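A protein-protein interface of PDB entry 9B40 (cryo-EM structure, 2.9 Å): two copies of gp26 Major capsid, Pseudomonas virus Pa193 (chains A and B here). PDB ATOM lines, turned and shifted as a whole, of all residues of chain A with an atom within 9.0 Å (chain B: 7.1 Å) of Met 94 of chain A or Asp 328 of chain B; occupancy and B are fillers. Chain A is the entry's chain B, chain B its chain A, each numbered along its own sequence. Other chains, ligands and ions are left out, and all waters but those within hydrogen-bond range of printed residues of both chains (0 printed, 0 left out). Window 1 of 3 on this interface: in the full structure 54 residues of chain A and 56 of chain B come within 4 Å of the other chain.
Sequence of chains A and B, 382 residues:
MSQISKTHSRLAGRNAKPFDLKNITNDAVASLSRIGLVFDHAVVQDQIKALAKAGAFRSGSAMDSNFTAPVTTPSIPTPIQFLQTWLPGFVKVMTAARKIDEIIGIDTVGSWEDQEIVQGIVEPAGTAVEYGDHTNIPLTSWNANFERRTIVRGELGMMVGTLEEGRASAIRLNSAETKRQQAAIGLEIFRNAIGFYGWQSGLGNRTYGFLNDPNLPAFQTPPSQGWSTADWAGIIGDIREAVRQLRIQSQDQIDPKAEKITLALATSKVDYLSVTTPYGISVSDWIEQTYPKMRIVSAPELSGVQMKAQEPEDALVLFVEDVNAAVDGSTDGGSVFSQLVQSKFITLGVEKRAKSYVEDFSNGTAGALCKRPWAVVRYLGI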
ATOM      1  N   PHE A  90      25.055  35.078 -25.892  1.00  0.00           N
ATOM      2  CA  PHE A  90      24.142  34.721 -26.966  1.00  0.00           C
ATOM      3  C   PHE A  90      23.831  33.237 -26.878  1.00  0.00           C
ATOM      4  O   PHE A  90      24.747  32.418 -26.752  1.00  0.00           O
ATOM      5  CB  PHE A  90      24.736  35.053 -28.337  1.00  0.00           C
ATOM      6  CG  PHE A  90      24.797  36.520 -28.633  1.00  0.00           C
ATOM      7  CD1 PHE A  90      25.871  37.283 -28.214  1.00  0.00           C
ATOM      8  CD2 PHE A  90      23.784  37.134 -29.347  1.00  0.00           C
ATOM      9  CE1 PHE A  90      25.926  38.633 -28.491  1.00  0.00           C
ATOM     10  CE2 PHE A  90      23.835  38.481 -29.630  1.00  0.00           C
ATOM     11  CZ  PHE A  90      24.907  39.231 -29.201  1.00  0.00           C
ATOM     12  N   VAL A  91      22.542  32.898 -26.923  1.00  0.00           N
ATOM     13  CA  VAL A  91      22.154  31.504 -27.072  1.00  0.00           C
ATOM     14  C   VAL A  91      22.650  31.010 -28.422  1.00  0.00           C
ATOM     15  O   VAL A  91      22.592  31.728 -29.426  1.00  0.00           O
ATOM     16  CB  VAL A  91      20.629  31.358 -26.935  1.00  0.00           C
ATOM     17  CG1 VAL A  91      20.206  29.907 -27.072  1.00  0.00           C
ATOM     18  CG2 VAL A  91      20.162  31.923 -25.608  1.00  0.00           C
ATOM     19  N   LYS A  92      23.180  29.792 -28.447  1.00  0.00           N
ATOM     20  CA  LYS A  92      23.728  29.213 -29.663  1.00  0.00           C
ATOM     21  C   LYS A  92      22.949  27.959 -30.018  1.00  0.00           C
ATOM     22  O   LYS A  92      22.646  27.143 -29.141  1.00  0.00           O
ATOM     23  CB  LYS A  92      25.217  28.897 -29.505  1.00  0.00           C
ATOM     24  CG  LYS A  92      26.122  29.858 -30.249  1.00  0.00           C
ATOM     25  CD  LYS A  92      27.485  29.947 -29.600  1.00  0.00           C
ATOM     26  CE  LYS A  92      28.177  31.246 -29.964  1.00  0.00           C
ATOM     27  NZ  LYS A  92      29.658  31.102 -29.961  1.00  0.00           N
ATOM     28  N   VAL A  93      22.603  27.828 -31.301  1.00  0.00           N
ATOM     29  CA  VAL A  93      21.935  26.628 -31.784  1.00  0.00           C
ATOM     30  C   VAL A  93      22.841  25.428 -31.564  1.00  0.00           C
ATOM     31  O   VAL A  93      24.050  25.485 -31.821  1.00  0.00           O
ATOM     32  CB  VAL A  93      21.554  26.800 -33.263  1.00  0.00           C
ATOM     33  CG1 VAL A  93      21.087  25.488 -33.865  1.00  0.00           C
ATOM     34  CG2 VAL A  93      20.470  27.853 -33.398  1.00  0.00           C
ATOM     35  N   MET A  94      22.269  24.346 -31.052  1.00  0.00           N
ATOM     36  CA  MET A  94      23.009  23.137 -30.739  1.00  0.00           C
ATOM     37  C   MET A  94      22.612  22.009 -31.680  1.00  0.00           C
ATOM     38  O   MET A  94      21.558  22.044 -32.321  1.00  0.00           O
ATOM     39  CB  MET A  94      22.767  22.715 -29.288  1.00  0.00           C
ATOM     40  CG  MET A  94      21.372  22.176 -29.035  1.00  0.00           C
ATOM     41  SD  MET A  94      21.307  21.044 -27.639  1.00  0.00           S
ATOM     42  CE  MET A  94      22.636  21.684 -26.632  1.00  0.00           C
ATOM     43  N   THR A  95      23.481  21.008 -31.764  1.00  0.00           N
ATOM     44  CA  THR A  95      23.239  19.808 -32.551  1.00  0.00           C
ATOM     45  C   THR A  95      23.109  18.601 -31.630  1.00  0.00           C
ATOM     46  O   THR A  95      23.087  18.724 -30.403  1.00  0.00           O
ATOM     47  CB  THR A  95      24.348  19.587 -33.580  1.00  0.00           C
ATOM     48  OG1 THR A  95      25.532  19.121 -32.919  1.00  0.00           O
ATOM     49  CG2 THR A  95      24.645  20.863 -34.328  1.00  0.00           C
ATOM     50  N   ALA A  96      23.004  17.426 -32.246  1.00  0.00           N
ATOM     51  CA  ALA A  96      22.819  16.189 -31.506  1.00  0.00           C
ATOM     52  C   ALA A  96      24.028  15.902 -30.621  1.00  0.00           C
ATOM     53  O   ALA A  96      25.136  16.390 -30.854  1.00  0.00           O
ATOM     54  CB  ALA A  96      22.585  15.023 -32.465  1.00  0.00           C
ATOM     55  N   ALA A  97      23.798  15.094 -29.590  1.00  0.00           N
ATOM     56  CA  ALA A  97      24.842  14.815 -28.617  1.00  0.00           C
ATOM     57  C   ALA A  97      25.939  13.956 -29.228  1.00  0.00           C
ATOM     58  O   ALA A  97      25.669  12.959 -29.902  1.00  0.00           O
ATOM     59  CB  ALA A  97      24.253  14.114 -27.396  1.00  0.00           C
ATOM     60  N   ARG A  98      27.182  14.357 -28.993  1.00  0.00           N
ATOM     61  CA  ARG A  98      28.352  13.597 -29.411  1.00  0.00           C
ATOM     62  C   ARG A  98      28.799  12.767 -28.214  1.00  0.00           C
ATOM     63  O   ARG A  98      29.351  13.305 -27.250  1.00  0.00           O
ATOM     64  CB  ARG A  98      29.459  14.527 -29.895  1.00  0.00           C
ATOM     65  CG  ARG A  98      29.031  15.449 -31.021  1.00  0.00           C
ATOM     66  CD  ARG A  98      30.008  16.593 -31.194  1.00  0.00           C
ATOM     67  NE  ARG A  98      29.334  17.883 -31.171  1.00  0.00           N
ATOM     68  CZ  ARG A  98      29.625  18.859 -30.323  1.00  0.00           C
ATOM     69  NH1 ARG A  98      30.573  18.720 -29.412  1.00  0.00           N
ATOM     70  NH2 ARG A  98      28.946  20.000 -30.388  1.00  0.00           N
ATOM     71  N   THR A 178      33.751  33.480 -32.374  1.00  0.00           N
ATOM     72  CA  THR A 178      32.632  32.581 -32.635  1.00  0.00           C
ATOM     73  C   THR A 178      32.882  31.733 -33.878  1.00  0.00           C
ATOM     74  O   THR A 178      32.532  30.548 -33.902  1.00  0.00           O
ATOM     75  CB  THR A 178      31.308  33.352 -32.733  1.00  0.00           C
ATOM     76  OG1 THR A 178      30.228  32.423 -32.891  1.00  0.00           O
ATOM     77  CG2 THR A 178      31.290  34.331 -33.888  1.00  0.00           C
ATOM     78  N   GLN A 181      35.444  28.992 -32.728  1.00  0.00           N
ATOM     79  CA  GLN A 181      34.840  27.927 -31.936  1.00  0.00           C
ATOM     80  C   GLN A 181      33.833  27.125 -32.753  1.00  0.00           C
ATOM     81  O   GLN A 181      33.644  25.934 -32.490  1.00  0.00           O
ATOM     82  CB  GLN A 181      34.203  28.484 -30.661  1.00  0.00           C
ATOM     83  CG  GLN A 181      33.034  29.417 -30.857  1.00  0.00           C
ATOM     84  CD  GLN A 181      32.716  30.204 -29.600  1.00  0.00           C
ATOM     85  OE1 GLN A 181      31.872  29.802 -28.799  1.00  0.00           O
ATOM     86  NE2 GLN A 181      33.396  31.329 -29.418  1.00  0.00           N
ATOM     87  N   GLN A 182      33.205  27.735 -33.763  1.00  0.00           N
ATOM     88  CA  GLN A 182      32.380  26.955 -34.680  1.00  0.00           C
ATOM     89  C   GLN A 182      33.235  26.008 -35.513  1.00  0.00           C
ATOM     90  O   GLN A 182      32.821  24.881 -35.795  1.00  0.00           O
ATOM     91  CB  GLN A 182      31.560  27.885 -35.577  1.00  0.00           C
ATOM     92  CG  GLN A 182      30.792  27.202 -36.717  1.00  0.00           C
ATOM     93  CD  GLN A 182      30.059  25.933 -36.295  1.00  0.00           C
ATOM     94  OE1 GLN A 182      29.403  25.889 -35.255  1.00  0.00           O
ATOM     95  NE2 GLN A 182      30.172  24.892 -37.110  1.00  0.00           N
ATOM     96  N   ILE A 185      33.926  23.146 -33.219  1.00  0.00           N
ATOM     97  CA  ILE A 185      32.758  22.291 -33.021  1.00  0.00           C
ATOM     98  C   ILE A 185      32.473  21.464 -34.274  1.00  0.00           C
ATOM     99  O   ILE A 185      32.072  20.298 -34.187  1.00  0.00           O
ATOM    100  CB  ILE A 185      31.550  23.144 -32.596  1.00  0.00           C
ATOM    101  CG1 ILE A 185      31.732  23.627 -31.158  1.00  0.00           C
ATOM    102  CG2 ILE A 185      30.265  22.355 -32.675  1.00  0.00           C
ATOM    103  CD1 ILE A 185      30.947  24.876 -30.834  1.00  0.00           C
ATOM    104  N   GLY A 186      32.679  22.047 -35.457  1.00  0.00           N
ATOM    105  CA  GLY A 186      32.526  21.283 -36.684  1.00  0.00           C
ATOM    106  C   GLY A 186      33.537  20.159 -36.800  1.00  0.00           C
ATOM    107  O   GLY A 186      33.197  19.044 -37.211  1.00  0.00           O
ATOM    108  N   ILE A 189      32.298  17.449 -34.565  1.00  0.00           N
ATOM    109  CA  ILE A 189      31.242  16.662 -35.201  1.00  0.00           C
ATOM    110  C   ILE A 189      31.847  15.660 -36.175  1.00  0.00           C
ATOM    111  O   ILE A 189      31.457  14.483 -36.210  1.00  0.00           O
ATOM    112  CB  ILE A 189      30.229  17.592 -35.897  1.00  0.00           C
ATOM    113  CG1 ILE A 189      29.332  18.277 -34.867  1.00  0.00           C
ATOM    114  CG2 ILE A 189      29.387  16.829 -36.908  1.00  0.00           C
ATOM    115  CD1 ILE A 189      28.678  19.537 -35.377  1.00  0.00           C
ATOM    116  N   ILE B 121      20.033  35.060 -30.245  1.00  0.00           N
ATOM    117  CA  ILE B 121      20.254  33.666 -30.609  1.00  0.00           C
ATOM    118  C   ILE B 121      21.134  33.652 -31.853  1.00  0.00           C
ATOM    119  O   ILE B 121      20.745  34.177 -32.903  1.00  0.00           O
ATOM    120  CB  ILE B 121      18.926  32.920 -30.843  1.00  0.00           C
ATOM    121  CG1 ILE B 121      19.137  31.593 -31.579  1.00  0.00           C
ATOM    122  CG2 ILE B 121      17.901  33.808 -31.539  1.00  0.00           C
ATOM    123  CD1 ILE B 121      19.917  30.563 -30.808  1.00  0.00           C
ATOM    124  N   VAL B 122      22.321  33.068 -31.734  1.00  0.00           N
ATOM    125  CA  VAL B 122      23.296  33.040 -32.817  1.00  0.00           C
ATOM    126  C   VAL B 122      23.402  31.605 -33.309  1.00  0.00           C
ATOM    127  O   VAL B 122      23.829  30.711 -32.569  1.00  0.00           O
ATOM    128  CB  VAL B 122      24.663  33.576 -32.372  1.00  0.00           C
ATOM    129  CG1 VAL B 122      25.729  33.229 -33.398  1.00  0.00           C
ATOM    130  CG2 VAL B 122      24.599  35.075 -32.161  1.00  0.00           C
ATOM    131  N   PRO B 124      25.447  29.224 -35.603  1.00  0.00           N
ATOM    132  CA  PRO B 124      26.676  29.109 -36.384  1.00  0.00           C
ATOM    133  C   PRO B 124      26.512  28.092 -37.509  1.00  0.00           C
ATOM    134  O   PRO B 124      25.519  27.370 -37.592  1.00  0.00           O
ATOM    135  CB  PRO B 124      27.696  28.633 -35.346  1.00  0.00           C
ATOM    136  CG  PRO B 124      26.888  27.842 -34.378  1.00  0.00           C
ATOM    137  CD  PRO B 124      25.485  28.396 -34.386  1.00  0.00           C
ATOM    138  N   SER B 250      15.252  16.541 -28.279  1.00  0.00           N
ATOM    139  CA  SER B 250      16.549  16.996 -27.805  1.00  0.00           C
ATOM    140  C   SER B 250      17.719  16.251 -28.432  1.00  0.00           C
ATOM    141  O   SER B 250      18.863  16.672 -28.233  1.00  0.00           O
ATOM    142  CB  SER B 250      16.608  16.861 -26.284  1.00  0.00           C
ATOM    143  OG  SER B 250      17.872  16.389 -25.862  1.00  0.00           O
ATOM    144  N   GLN B 253      20.227  14.869 -25.643  1.00  0.00           N
ATOM    145  CA  GLN B 253      20.956  15.796 -24.788  1.00  0.00           C
ATOM    146  C   GLN B 253      20.408  15.803 -23.367  1.00  0.00           C
ATOM    147  O   GLN B 253      20.426  16.838 -22.692  1.00  0.00           O
ATOM    148  CB  GLN B 253      20.939  17.207 -25.377  1.00  0.00           C
ATOM    149  CG  GLN B 253      21.649  17.357 -26.718  1.00  0.00           C
ATOM    150  CD  GLN B 253      23.133  17.636 -26.573  1.00  0.00           C
ATOM    151  OE1 GLN B 253      23.791  17.128 -25.666  1.00  0.00           O
ATOM    152  NE2 GLN B 253      23.667  18.454 -27.470  1.00  0.00           N
ATOM    153  N   VAL B 323      21.236  23.562 -19.691  1.00  0.00           N
ATOM    154  CA  VAL B 323      22.009  22.849 -20.698  1.00  0.00           C
ATOM    155  C   VAL B 323      23.445  23.340 -20.604  1.00  0.00           C
ATOM    156  O   VAL B 323      23.681  24.546 -20.476  1.00  0.00           O
ATOM    157  CB  VAL B 323      21.458  23.065 -22.119  1.00  0.00           C
ATOM    158  CG1 VAL B 323      22.120  22.106 -23.080  1.00  0.00           C
ATOM    159  CG2 VAL B 323      19.950  22.890 -22.144  1.00  0.00           C
ATOM    160  N   ASN B 324      24.397  22.411 -20.643  1.00  0.00           N
ATOM    161  CA  ASN B 324      25.796  22.786 -20.496  1.00  0.00           C
ATOM    162  C   ASN B 324      26.278  23.618 -21.684  1.00  0.00           C
ATOM    163  O   ASN B 324      25.738  23.546 -22.791  1.00  0.00           O
ATOM    164  CB  ASN B 324      26.660  21.531 -20.242  1.00  0.00           C
ATOM    165  CG  ASN B 324      26.781  20.582 -21.449  1.00  0.00           C
ATOM    166  OD1 ASN B 324      26.606  20.945 -22.606  1.00  0.00           O
ATOM    167  ND2 ASN B 324      27.098  19.329 -21.147  1.00  0.00           N
ATOM    168  N   ALA B 325      27.281  24.453 -21.428  1.00  0.00           N
ATOM    169  CA  ALA B 325      27.792  25.375 -22.431  1.00  0.00           C
ATOM    170  C   ALA B 325      28.890  24.774 -23.295  1.00  0.00           C
ATOM    171  O   ALA B 325      29.335  25.428 -24.244  1.00  0.00           O
ATOM    172  CB  ALA B 325      28.320  26.643 -21.754  1.00  0.00           C
ATOM    173  N   ALA B 326      29.343  23.557 -22.990  1.00  0.00           N
ATOM    174  CA  ALA B 326      30.488  22.996 -23.698  1.00  0.00           C
ATOM    175  C   ALA B 326      30.112  22.500 -25.090  1.00  0.00           C
ATOM    176  O   ALA B 326      30.883  22.672 -26.042  1.00  0.00           O
ATOM    177  CB  ALA B 326      31.106  21.866 -22.875  1.00  0.00           C
ATOM    178  N   VAL B 327      28.944  21.869 -25.227  1.00  0.00           N
ATOM    179  CA  VAL B 327      28.601  21.208 -26.484  1.00  0.00           C
ATOM    180  C   VAL B 327      28.293  22.224 -27.582  1.00  0.00           C
ATOM    181  O   VAL B 327      28.568  21.979 -28.762  1.00  0.00           O
ATOM    182  CB  VAL B 327      27.445  20.211 -26.271  1.00  0.00           C
ATOM    183  CG1 VAL B 327      27.850  19.154 -25.258  1.00  0.00           C
ATOM    184  CG2 VAL B 327      26.179  20.916 -25.814  1.00  0.00           C
ATOM    185  N   ASP B 328      27.710  23.371 -27.224  1.00  0.00           N
ATOM    186  CA  ASP B 328      27.280  24.345 -28.217  1.00  0.00           C
ATOM    187  C   ASP B 328      28.063  25.649 -28.195  1.00  0.00           C
ATOM    188  O   ASP B 328      27.988  26.405 -29.168  1.00  0.00           O
ATOM    189  CB  ASP B 328      25.788  24.662 -28.040  1.00  0.00           C
ATOM    190  CG  ASP B 328      25.433  25.016 -26.612  1.00  0.00           C
ATOM    191  OD1 ASP B 328      26.165  24.594 -25.693  1.00  0.00           O
ATOM    192  OD2 ASP B 328      24.416  25.712 -26.406  1.00  0.00           O
ATOM    193  N   GLY B 329      28.805  25.931 -27.130  1.00  0.00           N
ATOM    194  CA  GLY B 329      29.518  27.186 -27.032  1.00  0.00           C
ATOM    195  C   GLY B 329      28.678  28.368 -26.610  1.00  0.00           C
ATOM    196  O   GLY B 329      29.120  29.511 -26.776  1.00  0.00           O
ATOM    197  N   SER B 330      27.475  28.133 -26.089  1.00  0.00           N
ATOM    198  CA  SER B 330      26.621  29.223 -25.637  1.00  0.00           C
ATOM    199  C   SER B 330      27.245  29.938 -24.446  1.00  0.00           C
ATOM    200  O   SER B 330      27.756  29.308 -23.518  1.00  0.00           O
ATOM    201  CB  SER B 330      25.241  28.692 -25.253  1.00  0.00           C
ATOM    202  OG  SER B 330      24.451  28.429 -26.397  1.00  0.00           O
ATOM    203  N   THR B 331      27.194  31.268 -24.474  1.00  0.00           N
ATOM    204  CA  THR B 331      27.687  32.093 -23.380  1.00  0.00           C
ATOM    205  C   THR B 331      26.560  32.821 -22.658  1.00  0.00           C
ATOM    206  O   THR B 331      26.817  33.765 -21.906  1.00  0.00           O
ATOM    207  CB  THR B 331      28.721  33.092 -23.895  1.00  0.00           C
ATOM    208  OG1 THR B 331      28.948  34.102 -22.903  1.00  0.00           O
ATOM    209  CG2 THR B 331      28.241  33.738 -25.183  1.00  0.00           C
ATOM    210  N   ASP B 332      25.314  32.400 -22.876  1.00  0.00           N
ATOM    211  CA  ASP B 332      24.181  33.046 -22.224  1.00  0.00           C
ATOM    212  C   ASP B 332      24.042  32.630 -20.766  1.00  0.00           C
ATOM    213  O   ASP B 332      23.574  33.423 -19.944  1.00  0.00           O
ATOM    214  CB  ASP B 332      22.896  32.743 -23.000  1.00  0.00           C
ATOM    215  CG  ASP B 332      22.451  31.297 -22.868  1.00  0.00           C
ATOM    216  OD1 ASP B 332      21.798  30.954 -21.860  1.00  0.00           O
ATOM    217  OD2 ASP B 332      22.757  30.498 -23.778  1.00  0.00           O
ATOM    218  N   GLY B 334      23.193  29.021 -20.200  1.00  0.00           N
ATOM    219  CA  GLY B 334      22.805  27.642 -20.386  1.00  0.00           C
ATOM    220  C   GLY B 334      21.412  27.283 -19.919  1.00  0.00           C
ATOM    221  O   GLY B 334      20.978  26.147 -20.146  1.00  0.00           O
ATOM    222  N   ARG B 372      15.254  27.898 -25.008  1.00  0.00           N
ATOM    223  CA  ARG B 372      15.452  26.601 -25.653  1.00  0.00           C
ATOM    224  C   ARG B 372      14.104  25.896 -25.754  1.00  0.00           C
ATOM    225  O   ARG B 372      13.771  25.044 -24.920  1.00  0.00           O
ATOM    226  CB  ARG B 372      16.477  25.765 -24.890  1.00  0.00           C
ATOM    227  CG  ARG B 372      17.915  26.141 -25.208  1.00  0.00           C
ATOM    228  CD  ARG B 372      18.710  26.455 -23.958  1.00  0.00           C
ATOM    229  NE  ARG B 372      20.109  26.718 -24.270  1.00  0.00           N
ATOM    230  CZ  ARG B 372      20.773  27.797 -23.878  1.00  0.00           C
ATOM    231  NH1 ARG B 372      20.194  28.737 -23.151  1.00  0.00           N
ATOM    232  NH2 ARG B 372      22.050  27.934 -24.221  1.00  0.00           N
ATOM    233  N   TRP B 374      13.155  23.631 -27.764  1.00  0.00           N
ATOM    234  CA  TRP B 374      13.268  22.208 -28.071  1.00  0.00           C
ATOM    235  C   TRP B 374      13.219  21.353 -26.815  1.00  0.00           C
ATOM    236  O   TRP B 374      12.810  20.188 -26.871  1.00  0.00           O
ATOM    237  CB  TRP B 374      14.560  21.933 -28.840  1.00  0.00           C
ATOM    238  CG  TRP B 374      15.769  22.501 -28.179  1.00  0.00           C
ATOM    239  CD1 TRP B 374      16.297  23.740 -28.373  1.00  0.00           C
ATOM    240  CD2 TRP B 374      16.601  21.858 -27.206  1.00  0.00           C
ATOM    241  NE1 TRP B 374      17.408  23.909 -27.587  1.00  0.00           N
ATOM    242  CE2 TRP B 374      17.616  22.769 -26.860  1.00  0.00           C
ATOM    243  CE3 TRP B 374      16.589  20.600 -26.598  1.00  0.00           C
ATOM    244  CZ2 TRP B 374      18.605  22.465 -25.932  1.00  0.00           C
ATOM    245  CZ3 TRP B 374      17.574  20.300 -25.676  1.00  0.00           C
ATOM    246  CH2 TRP B 374      18.568  21.228 -25.352  1.00  0.00           C
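Among the printed residues, merely in contact across the chains: Phe 90 of chain A with Val 122 of chain B (3.6 Å), Phe 90 of chain A with Ser 330 of chain B (3.9 Å), Phe 90 of chain A with Thr 331 of chain B (3.5 Å), Phe 90 of chain A with Asp 332 of chain B (3.9 Å), Val 91 of chain A with Ile 121 of chain B (3.2 Å), Val 91 of chain A with Ser 330 of chain B (3.7 Å), Val 91 of chain A with Asp 332 of chain B (3.5 Å), Val 91 of chain A with Arg 372 of chain B (3.9 Å), Lys 92 of chain A with Val 122 of chain B (3.3 Å), Lys 92 of chain A with Asp 328 of chain B (3.6 Å), Lys 92 of chain A with Gly 329 of chain B (3.3 Å), Val 93 of chain A with Ile 121 of chain B (3.8 Å), Met 94 of chain A with Val 323 of chain B (3.6 Å), Met 94 of chain A with Val 327 of chain B (3.7 Å), Met 94 of chain A with Asp 328 of chain B (3.8 Å), Met 94 of chain A with Trp 374 of chain B (3.5 Å), Ala 97 of chain A with Gln 253 of chain B (3.5 Å), Gln 182 of chain A with Pro 124 of chain B (3.2 Å) and Ile 185 of chain A with Asp 328 of chain B (3.7 Å).
Hydrophobic or aromatic side chains of chain B that line the printed part of chain A: Ile 121, Val 122, Pro 124, Val 323, Val 327 and Trp 374.
Of the 15 printed residues of chain A, 11 touch a printed residue of chain B.
SD of Met 94 of chain A sits close to NE2 of Gln 253 of chain B (3.5 Å).
The side-chain hydroxyl of Ser 330 of chain B sits at hydrogen-bond distance from the backbone NH of Lys 92 of chain A (2.8 Å).
The side-chain amide nitrogen (NE2) of Gln 253 of chain B sits at hydrogen-bond distance from the backbone carbonyl oxygen (O) of Thr 95 of chain A, 3.0 Å away.
O of Val 91 of chain A sits at hydrogen-bond distance from N of Val 122 of chain B (2.7 Å).
O of Val 327 of chain B lies within hydrogen-bond range of NH2 of Arg 98 of chain A (2.6 Å).
The backbone carbonyl oxygen (O) of Gly 329 of chain B lies close to the side-chain amide oxygen (OE1) of Gln 181 of chain A (3.4 Å).
N of Val 93 of chain A is in hydrogen-bond range of O of Val 122 of chain B.
No position is printed for both chains.
Of the 26 pairs that touch across the chains among the printed residues, none has its exchanged pair printed and touching as well.
The side-chain carboxylate (OD2) of Asp 332 of chain B lies within salt-bridge range of the guanidinium group (NH2) of Arg 372 of chain B (2.7 Å).
NH2 of Arg 372 of chain B lies within salt-bridge range of OD2 of Asp 328 of chain B (3.9 Å).
The backbone NH of Val 323 of chain B sits at hydrogen-bond distance from the backbone carbonyl oxygen of Gly 334 of chain B (2.6 Å).
OD1 of Asp 332 of chain B is in hydrogen-bond range of N of Gly 334 of chain B, at 2.9 Å.
NH2 of Arg 372 of chain B sits at hydrogen-bond distance from OG of Ser 330 of chain B, at 3.3 Å.
The backbone NH of Gln 253 of chain B sits at hydrogen-bond distance from the side-chain hydroxyl of Ser 250 of chain B (2.8 Å).
Of the printed residues of chain B, Phe 90 of chain A touches Val 122 (3.6 Å), Ser 330 (3.9 Å), Thr 331 (3.5 Å) and Asp 332 (3.9 Å).
Of chain B, only Gln 253 (3.5 Å), Val 323 (3.6 Å), Val 327 (3.7 Å), Asp 328 (3.8 Å) and Trp 374 (3.5 Å) come within 4 Å of Met 94 of chain A.
Of the printed residues of chain A, Pro 124 of chain B touches Gln 182 (3.2 Å).
No residue of chain A comes within 4 Å of Ala 325 of chain B.
Of the printed residues of chain A, Val 327 of chain B touches Met 94 (3.7 Å) and Arg 98 (2.6 Å).
Of chain A, only Lys 92 (3.6 Å), Met 94 (3.8 Å) and Ile 185 (3.7 Å) come within 4 Å of Asp 328 of chain B.
Of chain A, only Lys 92 and Gln 181 come within 4 Å of Gly 329 of chain B.
Printed residues of chain A within 4 Å of Thr 331 of chain B: Phe 90.
The nearest residue of chain A that does not touch Asp 328 of chain B is Val 93 of chain A (4.2 Å).
The nearest printed residue of chain B that does not touch Val 91 of chain A is Thr 331 of chain B (5.5 Å).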
